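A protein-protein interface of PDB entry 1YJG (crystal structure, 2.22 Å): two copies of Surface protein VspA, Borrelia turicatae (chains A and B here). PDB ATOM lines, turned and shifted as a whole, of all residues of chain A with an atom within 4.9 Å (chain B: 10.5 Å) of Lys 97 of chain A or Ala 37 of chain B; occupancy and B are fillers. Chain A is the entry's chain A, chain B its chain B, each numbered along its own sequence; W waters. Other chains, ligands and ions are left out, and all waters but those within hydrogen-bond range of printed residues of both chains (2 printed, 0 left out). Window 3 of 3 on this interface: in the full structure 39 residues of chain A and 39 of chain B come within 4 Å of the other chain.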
ATOM      1  N   TYR A  55      16.292  33.656  33.818  1.00  0.00           N
ATOM      2  CA  TYR A  55      16.033  32.259  33.523  1.00  0.00           C
ATOM      3  C   TYR A  55      17.354  31.526  33.241  1.00  0.00           C
ATOM      4  O   TYR A  55      17.534  30.406  33.694  1.00  0.00           O
ATOM      5  CB  TYR A  55      15.092  32.136  32.319  1.00  0.00           C
ATOM      6  CG  TYR A  55      14.702  30.719  32.009  1.00  0.00           C
ATOM      7  CD1 TYR A  55      13.536  30.175  32.519  1.00  0.00           C
ATOM      8  CD2 TYR A  55      15.516  29.910  31.224  1.00  0.00           C
ATOM      9  CE1 TYR A  55      13.187  28.868  32.253  1.00  0.00           C
ATOM     10  CE2 TYR A  55      15.167  28.597  30.946  1.00  0.00           C
ATOM     11  CZ  TYR A  55      14.006  28.084  31.468  1.00  0.00           C
ATOM     12  OH  TYR A  55      13.655  26.786  31.204  1.00  0.00           O
ATOM     13  N   LEU A  93      12.247  27.159  36.985  1.00  0.00           N
ATOM     14  CA  LEU A  93      12.354  26.971  35.533  1.00  0.00           C
ATOM     15  C   LEU A  93      11.073  26.409  34.903  1.00  0.00           C
ATOM     16  O   LEU A  93      10.632  26.889  33.869  1.00  0.00           O
ATOM     17  CB  LEU A  93      13.545  26.066  35.189  1.00  0.00           C
ATOM     18  CG  LEU A  93      14.922  26.544  35.649  1.00  0.00           C
ATOM     19  CD1 LEU A  93      15.968  25.450  35.396  1.00  0.00           C
ATOM     20  CD2 LEU A  93      15.318  27.835  34.957  1.00  0.00           C
ATOM     21  N   THR A  94      10.481  25.402  35.540  1.00  0.00           N
ATOM     22  CA  THR A  94       9.255  24.780  35.054  1.00  0.00           C
ATOM     23  C   THR A  94       8.096  25.793  35.073  1.00  0.00           C
ATOM     24  O   THR A  94       7.311  25.878  34.125  1.00  0.00           O
ATOM     25  CB  THR A  94       8.904  23.549  35.938  1.00  0.00           C
ATOM     26  OG1 THR A  94       9.869  22.517  35.747  1.00  0.00           O
ATOM     27  CG2 THR A  94       7.603  22.889  35.507  1.00  0.00           C
ATOM     28  N   LYS A  95       8.004  26.555  36.157  1.00  0.00           N
ATOM     29  CA  LYS A  95       6.956  27.553  36.309  1.00  0.00           C
ATOM     30  C   LYS A  95       7.086  28.657  35.254  1.00  0.00           C
ATOM     31  O   LYS A  95       6.102  29.054  34.630  1.00  0.00           O
ATOM     32  CB  LYS A  95       6.979  28.132  37.738  1.00  0.00           C
ATOM     33  CG  LYS A  95       6.047  29.324  37.979  1.00  0.00           C
ATOM     34  CD  LYS A  95       4.590  29.073  37.546  1.00  0.00           C
ATOM     35  CE  LYS A  95       3.875  28.050  38.428  1.00  0.00           C
ATOM     36  NZ  LYS A  95       3.480  28.606  39.749  1.00  0.00           N
ATOM     37  N   ALA A  96       8.302  29.138  35.043  1.00  0.00           N
ATOM     38  CA  ALA A  96       8.536  30.196  34.066  1.00  0.00           C
ATOM     39  C   ALA A  96       8.147  29.728  32.657  1.00  0.00           C
ATOM     40  O   ALA A  96       7.455  30.442  31.916  1.00  0.00           O
ATOM     41  CB  ALA A  96       9.977  30.640  34.113  1.00  0.00           C
ATOM     42  N   LYS A  97       8.574  28.520  32.307  1.00  0.00           N
ATOM     43  CA  LYS A  97       8.278  27.934  30.999  1.00  0.00           C
ATOM     44  C   LYS A  97       6.772  27.832  30.793  1.00  0.00           C
ATOM     45  O   LYS A  97       6.272  28.096  29.698  1.00  0.00           O
ATOM     46  CB  LYS A  97       8.906  26.544  30.862  1.00  0.00           C
ATOM     47  CG  LYS A  97      10.384  26.551  30.505  1.00  0.00           C
ATOM     48  CD  LYS A  97      10.905  25.135  30.190  1.00  0.00           C
ATOM     49  CE  LYS A  97      10.967  24.250  31.427  1.00  0.00           C
ATOM     50  NZ  LYS A  97      11.822  23.046  31.218  1.00  0.00           N
ATOM     51  N   SER A  98       6.055  27.467  31.855  1.00  0.00           N
ATOM     52  CA  SER A  98       4.597  27.331  31.812  1.00  0.00           C
ATOM     53  C   SER A  98       3.910  28.685  31.659  1.00  0.00           C
ATOM     54  O   SER A  98       2.752  28.755  31.238  1.00  0.00           O
ATOM     55  CB  SER A  98       4.085  26.641  33.082  1.00  0.00           C
ATOM     56  OG  SER A  98       3.937  27.573  34.138  1.00  0.00           O
ATOM     57  N   LYS A  99       4.620  29.746  32.043  1.00  0.00           N
ATOM     58  CA  LYS A  99       4.122  31.118  31.956  1.00  0.00           C
ATOM     59  C   LYS A  99       4.727  31.846  30.748  1.00  0.00           C
ATOM     60  O   LYS A  99       4.823  33.065  30.742  1.00  0.00           O
ATOM     61  CB  LYS A  99       4.416  31.880  33.255  1.00  0.00           C
ATOM     62  CG  LYS A  99       3.675  31.334  34.472  1.00  0.00           C
ATOM     63  CD  LYS A  99       2.197  31.731  34.461  1.00  0.00           C
ATOM     64  CE  LYS A  99       1.390  30.991  35.523  1.00  0.00           C
ATOM     65  NZ  LYS A  99       0.006  31.532  35.571  1.00  0.00           N
ATOM     66  N   THR A 100       5.109  31.091  29.721  1.00  0.00           N
ATOM     67  CA  THR A 100       5.703  31.659  28.504  1.00  0.00           C
ATOM     68  C   THR A 100       4.846  32.722  27.815  1.00  0.00           C
ATOM     69  O   THR A 100       5.384  33.669  27.252  1.00  0.00           O
ATOM     70  CB  THR A 100       6.078  30.538  27.476  1.00  0.00           C
ATOM     71  OG1 THR A 100       6.558  31.134  26.267  1.00  0.00           O
ATOM     72  CG2 THR A 100       4.861  29.729  27.003  1.00  0.00           C
ATOM     73  N   LYS B  33      16.642  35.888  22.906  1.00  0.00           N
ATOM     74  CA  LYS B  33      15.955  34.690  23.380  1.00  0.00           C
ATOM     75  C   LYS B  33      14.810  35.041  24.323  1.00  0.00           C
ATOM     76  O   LYS B  33      14.904  35.961  25.131  1.00  0.00           O
ATOM     77  CB  LYS B  33      16.911  33.767  24.146  1.00  0.00           C
ATOM     78  CG  LYS B  33      18.108  33.238  23.377  1.00  0.00           C
ATOM     79  CD  LYS B  33      17.775  31.953  22.622  1.00  0.00           C
ATOM     80  CE  LYS B  33      18.883  31.582  21.651  1.00  0.00           C
ATOM     81  NZ  LYS B  33      20.203  31.508  22.338  1.00  0.00           N
ATOM     82  N   LYS B  34      13.717  34.304  24.201  1.00  0.00           N
ATOM     83  CA  LYS B  34      12.547  34.491  25.043  1.00  0.00           C
ATOM     84  C   LYS B  34      12.362  33.196  25.804  1.00  0.00           C
ATOM     85  O   LYS B  34      12.941  32.174  25.448  1.00  0.00           O
ATOM     86  CB  LYS B  34      11.297  34.784  24.206  1.00  0.00           C
ATOM     87  CG  LYS B  34      10.714  33.567  23.474  1.00  0.00           C
ATOM     88  CD  LYS B  34       9.456  33.922  22.694  1.00  0.00           C
ATOM     89  CE  LYS B  34       8.798  32.668  22.127  1.00  0.00           C
ATOM     90  NZ  LYS B  34       7.467  32.920  21.478  1.00  0.00           N
ATOM     91  N   ILE B  35      11.555  33.243  26.853  1.00  0.00           N
ATOM     92  CA  ILE B  35      11.283  32.061  27.640  1.00  0.00           C
ATOM     93  C   ILE B  35      10.134  31.383  26.911  1.00  0.00           C
ATOM     94  O   ILE B  35       9.019  31.907  26.871  1.00  0.00           O
ATOM     95  CB  ILE B  35      10.885  32.418  29.081  1.00  0.00           C
ATOM     96  CG1 ILE B  35      12.061  33.102  29.780  1.00  0.00           C
ATOM     97  CG2 ILE B  35      10.460  31.161  29.852  1.00  0.00           C
ATOM     98  CD1 ILE B  35      11.717  33.668  31.124  1.00  0.00           C
ATOM     99  N   GLY B  36      10.439  30.250  26.287  1.00  0.00           N
ATOM    100  CA  GLY B  36       9.461  29.469  25.546  1.00  0.00           C
ATOM    101  C   GLY B  36       8.942  28.345  26.418  1.00  0.00           C
ATOM    102  O   GLY B  36       9.343  28.226  27.570  1.00  0.00           O
ATOM    103  N   ALA B  37       8.074  27.506  25.860  1.00  0.00           N
ATOM    104  CA  ALA B  37       7.489  26.378  26.598  1.00  0.00           C
ATOM    105  C   ALA B  37       8.494  25.282  26.981  1.00  0.00           C
ATOM    106  O   ALA B  37       8.235  24.527  27.916  1.00  0.00           O
ATOM    107  CB  ALA B  37       6.320  25.765  25.806  1.00  0.00           C
ATOM    108  N   ASN B  38       9.616  25.195  26.266  1.00  0.00           N
ATOM    109  CA  ASN B  38      10.659  24.189  26.534  1.00  0.00           C
ATOM    110  C   ASN B  38      12.029  24.777  26.914  1.00  0.00           C
ATOM    111  O   ASN B  38      13.027  24.063  26.959  1.00  0.00           O
ATOM    112  CB  ASN B  38      10.820  23.278  25.315  1.00  0.00           C
ATOM    113  CG  ASN B  38       9.606  22.403  25.076  1.00  0.00           C
ATOM    114  OD1 ASN B  38       9.274  21.539  25.891  1.00  0.00           O
ATOM    115  ND2 ASN B  38       8.938  22.618  23.949  1.00  0.00           N
ATOM    116  N   GLY B  39      12.070  26.071  27.214  1.00  0.00           N
ATOM    117  CA  GLY B  39      13.308  26.742  27.581  1.00  0.00           C
ATOM    118  C   GLY B  39      13.538  27.952  26.706  1.00  0.00           C
ATOM    119  O   GLY B  39      12.619  28.408  26.034  1.00  0.00           O
ATOM    120  N   LEU B  40      14.759  28.475  26.711  1.00  0.00           N
ATOM    121  CA  LEU B  40      15.081  29.643  25.894  1.00  0.00           C
ATOM    122  C   LEU B  40      14.989  29.280  24.413  1.00  0.00           C
ATOM    123  O   LEU B  40      15.621  28.326  23.959  1.00  0.00           O
ATOM    124  CB  LEU B  40      16.484  30.180  26.204  1.00  0.00           C
ATOM    125  CG  LEU B  40      16.727  30.791  27.590  1.00  0.00           C
ATOM    126  CD1 LEU B  40      18.096  31.447  27.618  1.00  0.00           C
ATOM    127  CD2 LEU B  40      15.637  31.789  27.988  1.00  0.00           C
ATOM    128  N   GLU B  41      14.170  30.038  23.686  1.00  0.00           N
ATOM    129  CA  GLU B  41      13.956  29.853  22.253  1.00  0.00           C
ATOM    130  C   GLU B  41      14.323  31.144  21.545  1.00  0.00           C
ATOM    131  O   GLU B  41      14.203  32.226  22.121  1.00  0.00           O
ATOM    132  CB  GLU B  41      12.491  29.523  21.965  1.00  0.00           C
ATOM    133  CG  GLU B  41      12.171  28.037  21.958  1.00  0.00           C
ATOM    134  CD  GLU B  41      10.727  27.757  22.347  1.00  0.00           C
ATOM    135  OE1 GLU B  41       9.822  28.396  21.756  1.00  0.00           O
ATOM    136  OE2 GLU B  41      10.507  26.913  23.253  1.00  0.00           O
ATOM    137  N   THR B  42      14.745  31.029  20.290  1.00  0.00           N
ATOM    138  CA  THR B  42      15.132  32.186  19.492  1.00  0.00           C
ATOM    139  C   THR B  42      13.992  33.194  19.288  1.00  0.00           C
ATOM    140  O   THR B  42      12.878  32.829  18.922  1.00  0.00           O
ATOM    141  CB  THR B  42      15.671  31.729  18.114  1.00  0.00           C
ATOM    142  OG1 THR B  42      16.828  30.902  18.292  1.00  0.00           O
ATOM    143  CG2 THR B  42      16.190  32.914  17.308  1.00  0.00           C
HETATM  144  O   HOH W   1       9.450  21.455  29.372  1.00  0.00           O
HETATM  145  O   HOH W   2       5.605  34.080  24.144  1.00  0.00           O
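Of the 9 printed residues of chain A, 4 touch a printed residue of chain B. Hydrophobic or aromatic side chains of chain A within 4 Å of the printed part of chain B: Tyr 55. Hydrophobic or aromatic side chains of chain B that line the printed part of chain A: Ile 35 and Leu 40. Among the printed residues, no Asp or Glu carboxylate lies within 4 Å of a Lys or Arg side-chain nitrogen of the other chain.
No position is printed for both chains. Of the 11 pairs that touch across the chains among the printed residues, none has its exchanged pair printed and touching as well.
Among the printed residues, merely in contact across the chains: Tyr 55 of chain A with Ile 35 of chain B (3.9 Å), Tyr 55 of chain A with Gly 39 of chain B (3.6 Å), Tyr 55 of chain A with Leu 40 of chain B (3.7 Å), Ala 96 of chain A with Ile 35 of chain B (3.7 Å), Lys 97 of chain A with Gly 36 of chain B (3.5 Å), Lys 97 of chain A with Ala 37 of chain B (3.6 Å), Lys 97 of chain A with Asn 38 of chain B (3.5 Å), Lys 97 of chain A with Gly 39 of chain B (3.3 Å), Thr 100 of chain A with Gly 36 of chain B (3.4 Å) and Thr 100 of chain A with Ala 37 of chain B (3.95 Å).
The backbone carbonyl oxygen of Ile 35 of chain B lies within hydrogen-bond range of the side-chain hydroxyl of Thr 100 of chain A (2.6 Å).
Printed residues of chain B within 4 Å of Tyr 55 of chain A: Ile 35 (3.9 Å), Gly 39 (3.6 Å) and Leu 40 (3.7 Å). Leu 93 of chain A touches none of the printed residues of chain B. No residue of chain B comes within 4 Å of Thr 94 of chain A. Lys 97 of chain A touches just these residues of chain B: Gly 36, Ala 37, Asn 38 and Gly 39. No residue of chain B comes within 4 Å of Ser 98 of chain A. Of chain B, only Ile 35 (2.6 Å), Gly 36 (3.4 Å) and Ala 37 (3.95 Å) come within 4 Å of Thr 100 of chain A. Of the printed residues of chain A, Gly 36 of chain B touches Lys 97 and Thr 100. Ala 37 of chain B touches just these residues of chain A: Lys 97 (3.6 Å) and Thr 100 (3.95 Å). Printed residues of chain A within 4 Å of Asn 38 of chain B: Lys 97. Of the printed residues of chain A, Gly 39 of chain B touches Tyr 55 and Lys 97. Printed residues of chain A within 4 Å of Leu 40 of chain B: Tyr 55 (3.7 Å). Thr 42 of chain B touches none of the printed residues of chain A. The nearest residue of chain B that does not touch Lys 97 of chain A is Ile 35 of chain B (4.1 Å). The nearest printed residue of chain A that does not touch Ala 37 of chain B is Ser 98 of chain A (5.4 Å).
Water W2 lies within hydrogen-bond range of the backbone carbonyl oxygen of Thr 100 of chain A (3.1 Å) and the side-chain amino group of Lys 34 of chain B (3.5 Å). Water W1 lies within hydrogen-bond range of the side-chain amino group of Lys 97 of chain A (3.4 Å) and the side-chain amide oxygen of Asn 38 of chain B (3.5 Å).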
